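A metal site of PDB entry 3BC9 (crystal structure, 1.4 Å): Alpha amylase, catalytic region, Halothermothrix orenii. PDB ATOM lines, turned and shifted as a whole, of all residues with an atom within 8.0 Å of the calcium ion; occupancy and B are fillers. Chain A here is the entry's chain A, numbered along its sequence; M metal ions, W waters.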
ATOM      1  N   PHE A 411      13.468  25.050   7.818  1.00  0.00           N
ATOM      2  CA  PHE A 411      13.646  23.779   7.058  1.00  0.00           C
ATOM      3  C   PHE A 411      13.285  23.990   5.611  1.00  0.00           C
ATOM      4  O   PHE A 411      13.963  23.495   4.698  1.00  0.00           O
ATOM      5  CB  PHE A 411      12.824  22.643   7.561  1.00  0.00           C
ATOM      6  CG  PHE A 411      13.327  21.337   7.094  1.00  0.00           C
ATOM      7  CD1 PHE A 411      14.272  20.651   7.850  1.00  0.00           C
ATOM      8  CD2 PHE A 411      12.880  20.794   5.957  1.00  0.00           C
ATOM      9  CE1 PHE A 411      14.791  19.479   7.383  1.00  0.00           C
ATOM     10  CE2 PHE A 411      13.406  19.590   5.475  1.00  0.00           C
ATOM     11  CZ  PHE A 411      14.332  18.954   6.205  1.00  0.00           C
ATOM     12  N   ASP A 414      16.165  25.500   3.967  1.00  0.00           N
ATOM     13  CA  ASP A 414      17.157  24.412   3.723  1.00  0.00           C
ATOM     14  C   ASP A 414      16.779  23.704   2.405  1.00  0.00           C
ATOM     15  O   ASP A 414      17.656  23.369   1.598  1.00  0.00           O
ATOM     16  CB  ASP A 414      17.166  23.474   4.943  1.00  0.00           C
ATOM     17  CG  ASP A 414      18.314  22.450   5.007  1.00  0.00           C
ATOM     18  OD1 ASP A 414      19.161  22.418   4.125  1.00  0.00           O
ATOM     19  OD2 ASP A 414      18.344  21.661   6.006  1.00  0.00           O
ATOM     20  N   MET A 415      15.518  23.401   2.239  1.00  0.00           N
ATOM     21  CA  MET A 415      15.065  22.665   1.055  1.00  0.00           C
ATOM     22  C   MET A 415      15.333  23.358  -0.255  1.00  0.00           C
ATOM     23  O   MET A 415      15.313  22.690  -1.299  1.00  0.00           O
ATOM     24  CB  MET A 415      13.589  22.308   1.152  1.00  0.00           C
ATOM     25  CG  MET A 415      13.282  21.285   2.144  1.00  0.00           C
ATOM     26  SD  MET A 415      11.537  20.961   2.439  1.00  0.00           S
ATOM     27  CE  MET A 415      11.072  20.621   0.818  1.00  0.00           C
ATOM     28  N   ASN A 417      17.999  24.383  -1.697  1.00  0.00           N
ATOM     29  CA  ASN A 417      19.133  23.746  -2.417  1.00  0.00           C
ATOM     30  C   ASN A 417      19.313  22.310  -2.021  1.00  0.00           C
ATOM     31  O   ASN A 417      20.383  21.748  -2.365  1.00  0.00           O
ATOM     32  CB  ASN A 417      20.397  24.546  -2.266  1.00  0.00           C
ATOM     33  CG  ASN A 417      20.977  24.478  -0.897  1.00  0.00           C
ATOM     34  OD1 ASN A 417      20.360  23.911  -0.034  1.00  0.00           O
ATOM     35  ND2 ASN A 417      22.148  25.070  -0.684  1.00  0.00           N
ATOM     36  N   GLY A 418      18.306  21.652  -1.417  1.00  0.00           N
ATOM     37  CA  GLY A 418      18.301  20.312  -0.973  1.00  0.00           C
ATOM     38  C   GLY A 418      18.542  20.216   0.525  1.00  0.00           C
ATOM     39  O   GLY A 418      19.485  20.761   1.078  1.00  0.00           O
ATOM     40  N   ALA A 419      17.689  19.479   1.147  1.00  0.00           N
ATOM     41  CA  ALA A 419      17.744  19.171   2.554  1.00  0.00           C
ATOM     42  C   ALA A 419      17.799  17.666   2.811  1.00  0.00           C
ATOM     43  O   ALA A 419      17.624  16.850   1.851  1.00  0.00           O
ATOM     44  CB  ALA A 419      16.494  19.751   3.257  1.00  0.00           C
ATOM     45  N   TYR A 420      17.916  17.260   4.055  1.00  0.00           N
ATOM     46  CA  TYR A 420      17.849  15.885   4.416  1.00  0.00           C
ATOM     47  C   TYR A 420      16.405  15.581   4.871  1.00  0.00           C
ATOM     48  O   TYR A 420      15.978  15.916   5.969  1.00  0.00           O
ATOM     49  CB  TYR A 420      18.869  15.564   5.510  1.00  0.00           C
ATOM     50  CG  TYR A 420      19.034  14.063   5.651  1.00  0.00           C
ATOM     51  CD1 TYR A 420      19.950  13.375   4.826  1.00  0.00           C
ATOM     52  CD2 TYR A 420      18.302  13.283   6.530  1.00  0.00           C
ATOM     53  CE1 TYR A 420      20.088  12.019   4.942  1.00  0.00           C
ATOM     54  CE2 TYR A 420      18.470  11.874   6.602  1.00  0.00           C
ATOM     55  CZ  TYR A 420      19.362  11.291   5.790  1.00  0.00           C
ATOM     56  OH  TYR A 420      19.597   9.921   5.769  1.00  0.00           O
ATOM     57  N   MET A 421      15.611  15.142   3.893  1.00  0.00           N
ATOM     58  CA  MET A 421      14.124  15.231   4.050  1.00  0.00           C
ATOM     59  C   MET A 421      13.555  14.445   5.194  1.00  0.00           C
ATOM     60  O   MET A 421      12.527  14.830   5.739  1.00  0.00           O
ATOM     61  CB  MET A 421      13.491  14.751   2.729  1.00  0.00           C
ATOM     62  CG  MET A 421      13.610  15.754   1.664  1.00  0.00           C
ATOM     63  SD  MET A 421      12.875  17.351   1.825  1.00  0.00           S
ATOM     64  CE  MET A 421      11.126  16.792   1.596  1.00  0.00           C
ATOM     65  N   ALA A 422      14.216  13.357   5.630  1.00  0.00           N
ATOM     66  CA  ALA A 422      13.756  12.542   6.727  1.00  0.00           C
ATOM     67  C   ALA A 422      13.668  13.430   8.015  1.00  0.00           C
ATOM     68  O   ALA A 422      12.925  13.107   8.909  1.00  0.00           O
ATOM     69  CB  ALA A 422      14.717  11.380   6.967  1.00  0.00           C
ATOM     70  N   ARG A 462      10.085  24.619  -4.439  1.00  0.00           N
ATOM     71  CA  ARG A 462       9.534  23.581  -3.635  1.00  0.00           C
ATOM     72  C   ARG A 462       8.505  24.123  -2.608  1.00  0.00           C
ATOM     73  O   ARG A 462       8.217  23.503  -1.578  1.00  0.00           O
ATOM     74  CB  ARG A 462      10.582  22.755  -2.897  1.00  0.00           C
ATOM     75  CG  ARG A 462      11.566  22.046  -3.891  1.00  0.00           C
ATOM     76  CD  ARG A 462      12.572  21.159  -3.185  1.00  0.00           C
ATOM     77  NE  ARG A 462      13.454  20.469  -4.149  1.00  0.00           N
ATOM     78  CZ  ARG A 462      14.620  20.936  -4.565  1.00  0.00           C
ATOM     79  NH1 ARG A 462      15.142  22.064  -4.106  1.00  0.00           N
ATOM     80  NH2 ARG A 462      15.270  20.227  -5.485  1.00  0.00           N
ATOM     81  N   ASP A 516      14.089   9.133   3.781  1.00  0.00           N
ATOM     82  CA  ASP A 516      15.465   9.182   3.401  1.00  0.00           C
ATOM     83  C   ASP A 516      15.918  10.593   3.091  1.00  0.00           C
ATOM     84  O   ASP A 516      15.246  11.568   3.422  1.00  0.00           O
ATOM     85  CB  ASP A 516      15.768   8.181   2.280  1.00  0.00           C
ATOM     86  CG  ASP A 516      15.070   8.457   0.968  1.00  0.00           C
ATOM     87  OD1 ASP A 516      14.889   9.621   0.600  1.00  0.00           O
ATOM     88  OD2 ASP A 516      14.787   7.455   0.174  1.00  0.00           O
ATOM     89  N   ALA A 517      17.066  10.773   2.503  1.00  0.00           N
ATOM     90  CA  ALA A 517      17.562  12.079   2.188  1.00  0.00           C
ATOM     91  C   ALA A 517      16.668  12.932   1.289  1.00  0.00           C
ATOM     92  O   ALA A 517      16.749  14.182   1.287  1.00  0.00           O
ATOM     93  CB  ALA A 517      18.980  12.034   1.571  1.00  0.00           C
ATOM     94  N   ASP A 518      15.905  12.212   0.433  1.00  0.00           N
ATOM     95  CA  ASP A 518      15.129  12.894  -0.610  1.00  0.00           C
ATOM     96  C   ASP A 518      13.623  12.722  -0.527  1.00  0.00           C
ATOM     97  O   ASP A 518      12.932  13.504  -1.228  1.00  0.00           O
ATOM     98  CB  ASP A 518      15.614  12.589  -2.013  1.00  0.00           C
ATOM     99  CG  ASP A 518      17.071  13.005  -2.255  1.00  0.00           C
ATOM    100  OD1 ASP A 518      17.664  13.824  -1.525  1.00  0.00           O
ATOM    101  OD2 ASP A 518      17.686  12.428  -3.183  1.00  0.00           O
ATOM    102  N   ILE A 519      13.119  11.834   0.282  1.00  0.00           N
ATOM    103  CA  ILE A 519      11.650  11.577   0.421  1.00  0.00           C
ATOM    104  C   ILE A 519      11.228  11.558   1.876  1.00  0.00           C
ATOM    105  O   ILE A 519      11.860  10.941   2.739  1.00  0.00           O
ATOM    106  CB  ILE A 519      11.217  10.254  -0.243  1.00  0.00           C
ATOM    107  CG1 ILE A 519      11.456  10.330  -1.752  1.00  0.00           C
ATOM    108  CG2 ILE A 519       9.746   9.940   0.106  1.00  0.00           C
ATOM    109  CD1 ILE A 519      11.213   8.987  -2.470  1.00  0.00           C
ATOM    110  N   SER A 540       9.116  15.264  -1.911  1.00  0.00           N
ATOM    111  CA  SER A 540      10.522  14.987  -2.240  1.00  0.00           C
ATOM    112  C   SER A 540      11.248  16.217  -2.719  1.00  0.00           C
ATOM    113  O   SER A 540      10.671  17.083  -3.397  1.00  0.00           O
ATOM    114  CB  SER A 540      10.619  13.872  -3.309  1.00  0.00           C
ATOM    115  OG  SER A 540      11.976  13.578  -3.675  1.00  0.00           O
ATOM    116  N   ASP A 541      12.532  16.311  -2.338  1.00  0.00           N
ATOM    117  CA  ASP A 541      13.392  17.336  -2.883  1.00  0.00           C
ATOM    118  C   ASP A 541      14.288  16.806  -4.027  1.00  0.00           C
ATOM    119  O   ASP A 541      15.192  17.509  -4.480  1.00  0.00           O
ATOM    120  CB  ASP A 541      14.219  18.053  -1.834  1.00  0.00           C
ATOM    121  CG  ASP A 541      15.286  17.166  -1.188  1.00  0.00           C
ATOM    122  OD1 ASP A 541      16.051  17.763  -0.394  1.00  0.00           O
ATOM    123  OD2 ASP A 541      15.365  15.947  -1.384  1.00  0.00           O
ATOM    124  N   GLY A 542      13.958  15.618  -4.501  1.00  0.00           N
ATOM    125  CA  GLY A 542      14.682  15.012  -5.614  1.00  0.00           C
ATOM    126  C   GLY A 542      14.507  15.746  -6.921  1.00  0.00           C
ATOM    127  O   GLY A 542      13.537  16.492  -7.149  1.00  0.00           O
ATOM    128  N   THR A 543      15.457  15.573  -7.846  1.00  0.00           N
ATOM    129  CA  THR A 543      15.404  16.262  -9.109  1.00  0.00           C
ATOM    130  C   THR A 543      15.691  15.319 -10.285  1.00  0.00           C
ATOM    131  O   THR A 543      15.846  15.808 -11.395  1.00  0.00           O
ATOM    132  CB  THR A 543      16.407  17.392  -9.176  1.00  0.00           C
ATOM    133  OG1 THR A 543      17.715  16.857  -8.964  1.00  0.00           O
ATOM    134  CG2 THR A 543      16.089  18.509  -8.107  1.00  0.00           C
HETATM  135 CA    CA M   1      17.545  15.816  -0.200  1.00  0.00          CA
HETATM  136  O   HOH W   1      18.592  16.941  -1.953  1.00  0.00           O
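Along chain A the residues within 4 Å of the calcium ion span positions 419 to 541.
O of Ala 517 lies close to N of Met 421 (3.0 Å). OD1 of Asp 516 sits at hydrogen-bond distance from N of Asp 518 (2.8 Å). O of Asp 518 sits at hydrogen-bond distance from OG of Ser 540, 2.6 Å away. NH2 of Arg 462 sits at hydrogen-bond distance from O of Asp 541, 2.9 Å away.
The calcium ion is bound by the backbone carbonyl oxygen (O) of Ala 419 (2.3 Å), water W1 (2.3 Å), the backbone carbonyl oxygen (O) of Ala 517 (2.3 Å), the side-chain carboxylate (OD1) of Asp 518 (2.4 Å), the side-chain carboxylate (OD1) of Asp 541 (2.5 Å) and the side-chain carboxylate (OD2) of Asp 541 (2.5 Å). The calcium ion has six donor atoms within binding distance.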
